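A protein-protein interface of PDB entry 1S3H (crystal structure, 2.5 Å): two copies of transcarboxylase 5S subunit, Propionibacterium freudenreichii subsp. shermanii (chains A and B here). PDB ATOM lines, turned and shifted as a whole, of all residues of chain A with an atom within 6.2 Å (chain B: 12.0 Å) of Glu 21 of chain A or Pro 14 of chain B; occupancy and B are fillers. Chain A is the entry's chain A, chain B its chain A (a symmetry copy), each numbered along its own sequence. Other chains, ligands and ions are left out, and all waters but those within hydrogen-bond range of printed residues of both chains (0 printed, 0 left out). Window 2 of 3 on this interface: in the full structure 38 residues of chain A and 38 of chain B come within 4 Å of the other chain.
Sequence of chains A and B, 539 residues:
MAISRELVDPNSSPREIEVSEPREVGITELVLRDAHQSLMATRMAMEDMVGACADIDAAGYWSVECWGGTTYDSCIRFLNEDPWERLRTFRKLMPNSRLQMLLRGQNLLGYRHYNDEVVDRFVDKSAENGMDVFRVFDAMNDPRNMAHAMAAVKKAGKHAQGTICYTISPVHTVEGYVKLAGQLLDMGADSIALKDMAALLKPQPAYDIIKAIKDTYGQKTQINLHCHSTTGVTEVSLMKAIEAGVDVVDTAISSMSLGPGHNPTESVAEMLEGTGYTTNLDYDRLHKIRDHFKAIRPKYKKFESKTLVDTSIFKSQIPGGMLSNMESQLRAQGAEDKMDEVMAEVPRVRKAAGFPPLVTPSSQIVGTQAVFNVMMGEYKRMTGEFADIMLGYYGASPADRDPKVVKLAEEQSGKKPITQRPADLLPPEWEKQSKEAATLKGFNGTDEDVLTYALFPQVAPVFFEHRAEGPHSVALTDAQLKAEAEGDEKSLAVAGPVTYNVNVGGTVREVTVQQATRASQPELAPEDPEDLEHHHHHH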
ATOM      1  N   GLU A  18      24.951   2.244  -4.217  1.00  0.00           N
ATOM      2  CA  GLU A  18      24.488   1.266  -3.222  1.00  0.00           C
ATOM      3  C   GLU A  18      25.663   0.807  -2.360  1.00  0.00           C
ATOM      4  O   GLU A  18      26.734   0.471  -2.865  1.00  0.00           O
ATOM      5  CB  GLU A  18      23.884   0.085  -3.948  1.00  0.00           C
ATOM      6  CG  GLU A  18      23.568  -1.070  -3.051  1.00  0.00           C
ATOM      7  CD  GLU A  18      22.554  -1.970  -3.672  1.00  0.00           C
ATOM      8  OE1 GLU A  18      21.352  -1.713  -3.465  1.00  0.00           O
ATOM      9  OE2 GLU A  18      22.955  -2.910  -4.384  1.00  0.00           O
ATOM     10  N   VAL A  19      25.457   0.781  -1.054  1.00  0.00           N
ATOM     11  CA  VAL A  19      26.530   0.345  -0.153  1.00  0.00           C
ATOM     12  C   VAL A  19      25.988  -0.725   0.797  1.00  0.00           C
ATOM     13  O   VAL A  19      24.793  -0.775   1.081  1.00  0.00           O
ATOM     14  CB  VAL A  19      27.100   1.520   0.634  1.00  0.00           C
ATOM     15  CG1 VAL A  19      27.884   2.405  -0.312  1.00  0.00           C
ATOM     16  CG2 VAL A  19      25.984   2.293   1.299  1.00  0.00           C
ATOM     17  N   SER A  20      26.878  -1.579   1.276  1.00  0.00           N
ATOM     18  CA  SER A  20      26.444  -2.673   2.153  1.00  0.00           C
ATOM     19  C   SER A  20      25.995  -2.100   3.497  1.00  0.00           C
ATOM     20  O   SER A  20      26.428  -1.028   3.918  1.00  0.00           O
ATOM     21  CB  SER A  20      27.570  -3.688   2.350  1.00  0.00           C
ATOM     22  OG  SER A  20      28.661  -3.138   3.063  1.00  0.00           O
ATOM     23  N   GLU A  21      25.104  -2.844   4.126  1.00  0.00           N
ATOM     24  CA  GLU A  21      24.527  -2.515   5.437  1.00  0.00           C
ATOM     25  C   GLU A  21      25.644  -2.320   6.463  1.00  0.00           C
ATOM     26  O   GLU A  21      26.735  -2.874   6.330  1.00  0.00           O
ATOM     27  CB  GLU A  21      23.627  -3.677   5.875  1.00  0.00           C
ATOM     28  CG  GLU A  21      24.360  -5.031   5.990  1.00  0.00           C
ATOM     29  CD  GLU A  21      24.873  -5.589   4.652  1.00  0.00           C
ATOM     30  OE1 GLU A  21      25.559  -6.635   4.675  1.00  0.00           O
ATOM     31  OE2 GLU A  21      24.597  -5.009   3.579  1.00  0.00           O
ATOM     32  N   PRO A  22      25.385  -1.513   7.499  1.00  0.00           N
ATOM     33  CA  PRO A  22      26.378  -1.263   8.551  1.00  0.00           C
ATOM     34  C   PRO A  22      26.830  -2.639   9.043  1.00  0.00           C
ATOM     35  O   PRO A  22      26.019  -3.560   9.113  1.00  0.00           O
ATOM     36  CB  PRO A  22      25.570  -0.525   9.605  1.00  0.00           C
ATOM     37  CG  PRO A  22      24.602   0.251   8.765  1.00  0.00           C
ATOM     38  CD  PRO A  22      24.151  -0.749   7.741  1.00  0.00           C
ATOM     39  N   ARG A  23      28.102  -2.790   9.397  1.00  0.00           N
ATOM     40  CA  ARG A  23      28.571  -4.112   9.838  1.00  0.00           C
ATOM     41  C   ARG A  23      30.048  -4.042  10.225  1.00  0.00           C
ATOM     42  O   ARG A  23      30.727  -3.053   9.955  1.00  0.00           O
ATOM     43  CB  ARG A  23      28.433  -5.093   8.676  1.00  0.00           C
ATOM     44  CG  ARG A  23      29.271  -4.643   7.502  1.00  0.00           C
ATOM     45  CD  ARG A  23      28.960  -5.378   6.215  1.00  0.00           C
ATOM     46  NE  ARG A  23      29.743  -4.815   5.123  1.00  0.00           N
ATOM     47  CZ  ARG A  23      30.926  -5.282   4.769  1.00  0.00           C
ATOM     48  NH1 ARG A  23      31.422  -6.312   5.424  1.00  0.00           N
ATOM     49  NH2 ARG A  23      31.613  -4.719   3.778  1.00  0.00           N
ATOM     50  N   GLN A 219      25.807 -13.201  -0.672  1.00  0.00           N
ATOM     51  CA  GLN A 219      26.432 -12.431   0.412  1.00  0.00           C
ATOM     52  C   GLN A 219      27.227 -13.313   1.380  1.00  0.00           C
ATOM     53  O   GLN A 219      28.201 -12.854   1.973  1.00  0.00           O
ATOM     54  CB  GLN A 219      25.356 -11.676   1.187  1.00  0.00           C
ATOM     55  CG  GLN A 219      24.472 -10.778   0.323  1.00  0.00           C
ATOM     56  CD  GLN A 219      23.775  -9.699   1.150  1.00  0.00           C
ATOM     57  OE1 GLN A 219      22.751  -9.147   0.749  1.00  0.00           O
ATOM     58  NE2 GLN A 219      24.354  -9.388   2.319  1.00  0.00           N
ATOM     59  N   GLU A 243      32.358  -0.903   0.913  1.00  0.00           N
ATOM     60  CA  GLU A 243      31.005  -0.464   0.544  1.00  0.00           C
ATOM     61  C   GLU A 243      30.356  -1.543  -0.323  1.00  0.00           C
ATOM     62  O   GLU A 243      29.143  -1.743  -0.268  1.00  0.00           O
ATOM     63  CB  GLU A 243      31.050   0.857  -0.223  1.00  0.00           C
ATOM     64  CG  GLU A 243      31.678   1.985   0.577  1.00  0.00           C
ATOM     65  CD  GLU A 243      31.836   3.258  -0.215  1.00  0.00           C
ATOM     66  OE1 GLU A 243      32.194   3.198  -1.412  1.00  0.00           O
ATOM     67  OE2 GLU A 243      31.616   4.333   0.369  1.00  0.00           O
ATOM     68  N   GLY A 276      29.232   3.712   9.485  1.00  0.00           N
ATOM     69  CA  GLY A 276      28.266   2.662   9.757  1.00  0.00           C
ATOM     70  C   GLY A 276      29.048   1.361   9.697  1.00  0.00           C
ATOM     71  O   GLY A 276      28.565   0.287  10.055  1.00  0.00           O
ATOM     72  N   TYR A 277      30.274   1.456   9.196  1.00  0.00           N
ATOM     73  CA  TYR A 277      31.159   0.285   9.142  1.00  0.00           C
ATOM     74  C   TYR A 277      32.096   0.380  10.347  1.00  0.00           C
ATOM     75  O   TYR A 277      32.452   1.477  10.770  1.00  0.00           O
ATOM     76  CB  TYR A 277      31.974   0.290   7.860  1.00  0.00           C
ATOM     77  CG  TYR A 277      31.115   0.269   6.643  1.00  0.00           C
ATOM     78  CD1 TYR A 277      31.213   1.275   5.689  1.00  0.00           C
ATOM     79  CD2 TYR A 277      30.203  -0.762   6.437  1.00  0.00           C
ATOM     80  CE1 TYR A 277      30.434   1.260   4.553  1.00  0.00           C
ATOM     81  CE2 TYR A 277      29.411  -0.794   5.302  1.00  0.00           C
ATOM     82  CZ  TYR A 277      29.536   0.221   4.356  1.00  0.00           C
ATOM     83  OH  TYR A 277      28.808   0.167   3.197  1.00  0.00           O
ATOM     84  N   PRO B  14      20.949  -3.066   2.417  1.00  0.00           N
ATOM     85  CA  PRO B  14      21.731  -2.203   1.488  1.00  0.00           C
ATOM     86  C   PRO B  14      21.121  -0.822   1.236  1.00  0.00           C
ATOM     87  O   PRO B  14      20.129  -0.659   0.525  1.00  0.00           O
ATOM     88  CB  PRO B  14      21.907  -2.986   0.193  1.00  0.00           C
ATOM     89  CG  PRO B  14      21.960  -4.419   0.744  1.00  0.00           C
ATOM     90  CD  PRO B  14      20.881  -4.441   1.882  1.00  0.00           C
ATOM     91  N   ARG B  15      21.759   0.158   1.868  1.00  0.00           N
ATOM     92  CA  ARG B  15      21.382   1.575   1.795  1.00  0.00           C
ATOM     93  C   ARG B  15      22.012   2.206   0.554  1.00  0.00           C
ATOM     94  O   ARG B  15      22.568   1.511  -0.295  1.00  0.00           O
ATOM     95  CB  ARG B  15      21.830   2.248   3.091  1.00  0.00           C
ATOM     96  CG  ARG B  15      23.219   1.821   3.499  1.00  0.00           C
ATOM     97  CD  ARG B  15      23.503   2.064   4.962  1.00  0.00           C
ATOM     98  NE  ARG B  15      24.806   1.510   5.272  1.00  0.00           N
ATOM     99  CZ  ARG B  15      25.897   2.228   5.499  1.00  0.00           C
ATOM    100  NH1 ARG B  15      25.857   3.553   5.473  1.00  0.00           N
ATOM    101  NH2 ARG B  15      27.046   1.614   5.707  1.00  0.00           N
ATOM    102  N   GLU B  16      21.950   3.523   0.456  1.00  0.00           N
ATOM    103  CA  GLU B  16      22.469   4.158  -0.761  1.00  0.00           C
ATOM    104  C   GLU B  16      23.152   5.481  -0.411  1.00  0.00           C
ATOM    105  O   GLU B  16      22.800   6.136   0.569  1.00  0.00           O
ATOM    106  CB  GLU B  16      21.286   4.384  -1.682  1.00  0.00           C
ATOM    107  CG  GLU B  16      21.618   4.545  -3.130  1.00  0.00           C
ATOM    108  CD  GLU B  16      20.668   3.723  -3.986  1.00  0.00           C
ATOM    109  OE1 GLU B  16      21.000   2.555  -4.324  1.00  0.00           O
ATOM    110  OE2 GLU B  16      19.571   4.249  -4.295  1.00  0.00           O
ATOM    111  N   ILE B  17      24.138   5.868  -1.204  1.00  0.00           N
ATOM    112  CA  ILE B  17      24.842   7.132  -0.951  1.00  0.00           C
ATOM    113  C   ILE B  17      24.806   7.995  -2.214  1.00  0.00           C
ATOM    114  O   ILE B  17      25.223   7.572  -3.291  1.00  0.00           O
ATOM    115  CB  ILE B  17      26.304   6.908  -0.568  1.00  0.00           C
ATOM    116  CG1 ILE B  17      26.374   6.198   0.776  1.00  0.00           C
ATOM    117  CG2 ILE B  17      27.027   8.241  -0.496  1.00  0.00           C
ATOM    118  CD1 ILE B  17      27.774   6.000   1.262  1.00  0.00           C
ATOM    119  N   GLU B  18      24.297   9.206  -2.051  1.00  0.00           N
ATOM    120  CA  GLU B  18      24.196  10.166  -3.159  1.00  0.00           C
ATOM    121  C   GLU B  18      25.583  10.706  -3.507  1.00  0.00           C
ATOM    122  O   GLU B  18      26.353  11.100  -2.632  1.00  0.00           O
ATOM    123  CB  GLU B  18      23.288  11.299  -2.738  1.00  0.00           C
ATOM    124  CG  GLU B  18      23.275  12.445  -3.701  1.00  0.00           C
ATOM    125  CD  GLU B  18      22.047  13.274  -3.531  1.00  0.00           C
ATOM    126  OE1 GLU B  18      21.036  12.947  -4.182  1.00  0.00           O
ATOM    127  OE2 GLU B  18      22.085  14.228  -2.731  1.00  0.00           O
ATOM    128  N   GLN B 204      33.675  10.304   6.453  1.00  0.00           N
ATOM    129  CA  GLN B 204      32.257  10.674   6.568  1.00  0.00           C
ATOM    130  C   GLN B 204      32.137  12.185   6.782  1.00  0.00           C
ATOM    131  O   GLN B 204      31.326  12.850   6.141  1.00  0.00           O
ATOM    132  CB  GLN B 204      31.574   9.931   7.717  1.00  0.00           C
ATOM    133  CG  GLN B 204      30.067  10.063   7.645  1.00  0.00           C
ATOM    134  CD  GLN B 204      29.556   9.562   6.301  1.00  0.00           C
ATOM    135  OE1 GLN B 204      29.810   8.417   5.927  1.00  0.00           O
ATOM    136  NE2 GLN B 204      28.842  10.421   5.566  1.00  0.00           N
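The guanidinium group (NH2) of Arg 15 of chain B lies close to the side-chain hydroxyl (OH) of Tyr 277 of chain A. NH2 of Arg 15 of chain B sits at hydrogen-bond distance from O of Ser 20 of chain A, 3.3 Å away. N of Val 19 of chain A sits at hydrogen-bond distance from O of Arg 15 of chain B (3.1 Å).
The side-chain hydroxyl of Ser 20 of chain A is in hydrogen-bond range of the guanidinium group of Arg 23 of chain A, 2.9 Å away. The backbone carbonyl oxygen (O) of Ser 20 of chain A sits at hydrogen-bond distance from the side-chain hydroxyl (OH) of Tyr 277 of chain A, 2.8 Å away. The backbone carbonyl oxygen of Glu 243 of chain A is in hydrogen-bond range of the backbone NH of Ser 20 of chain A (2.7 Å).
Pro 14 of chain B touches Glu 18 of chain A (CB to OE1, 3.9 Å). Glu 18 of chain A touches Arg 15 of chain B (CA to O, 3.5 Å). Glu 18 of chain A touches Glu 16 of chain B (CB to OE1, 3.8 Å). CA of Pro 14 of chain B touches O of Val 19 of chain A, 3.4 Å away. Ile 17 of chain B touches Val 19 of chain A. Pro 14 of chain B touches Glu 21 of chain A. Pro 22 of chain A touches Arg 15 of chain B (CD to NE, 3.4 Å).
Glu 21 of chain A touches just one residue of chain B: Pro 14. Pro 14 of chain B touches three residues of chain A. Of chain B, only Pro 14, Arg 15 and Ile 17 come within 4 Å of Val 19 of chain A. No residue of chain B comes within 4 Å of Gly 276 of chain A. Of the printed residues of chain A, Ile 17 of chain B touches Val 19. Printed residues of chain B within 4 Å of Tyr 277 of chain A: Arg 15 (3.2 Å). Of the printed residues of chain A, Arg 15 of chain B touches Glu 18, Val 19, Ser 20, Pro 22 and Tyr 277. Printed residues of chain A within 4 Å of Glu 16 of chain B: Glu 18 (3.8 Å). Glu 243 of chain A touches none of the printed residues of chain B. The nearest residue of chain B that does not touch Glu 21 of chain A is Arg 15 of chain B (4.04 Å). The nearest residue of chain A that does not touch Pro 14 of chain B is Ser 20 of chain A (4.7 Å).
Of the 6 printed residues of chain B, 4 touch a printed residue of chain A. Hydrophobic or aromatic side chains of chain B within 4 Å of the printed part of chain A: Pro 14 and Ile 17. Along chain B the printed residues that touch a printed residue of chain A span positions 14 to 17. Of the 10 printed residues of chain A, 6 touch a printed residue of chain B. Among the printed residues, 10 pairs touch across the chains. Among the printed residues, no Asp or Glu carboxylate lies within 4 Å of a Lys or Arg side-chain nitrogen of the other chain.
Position printed for both chains: 18.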
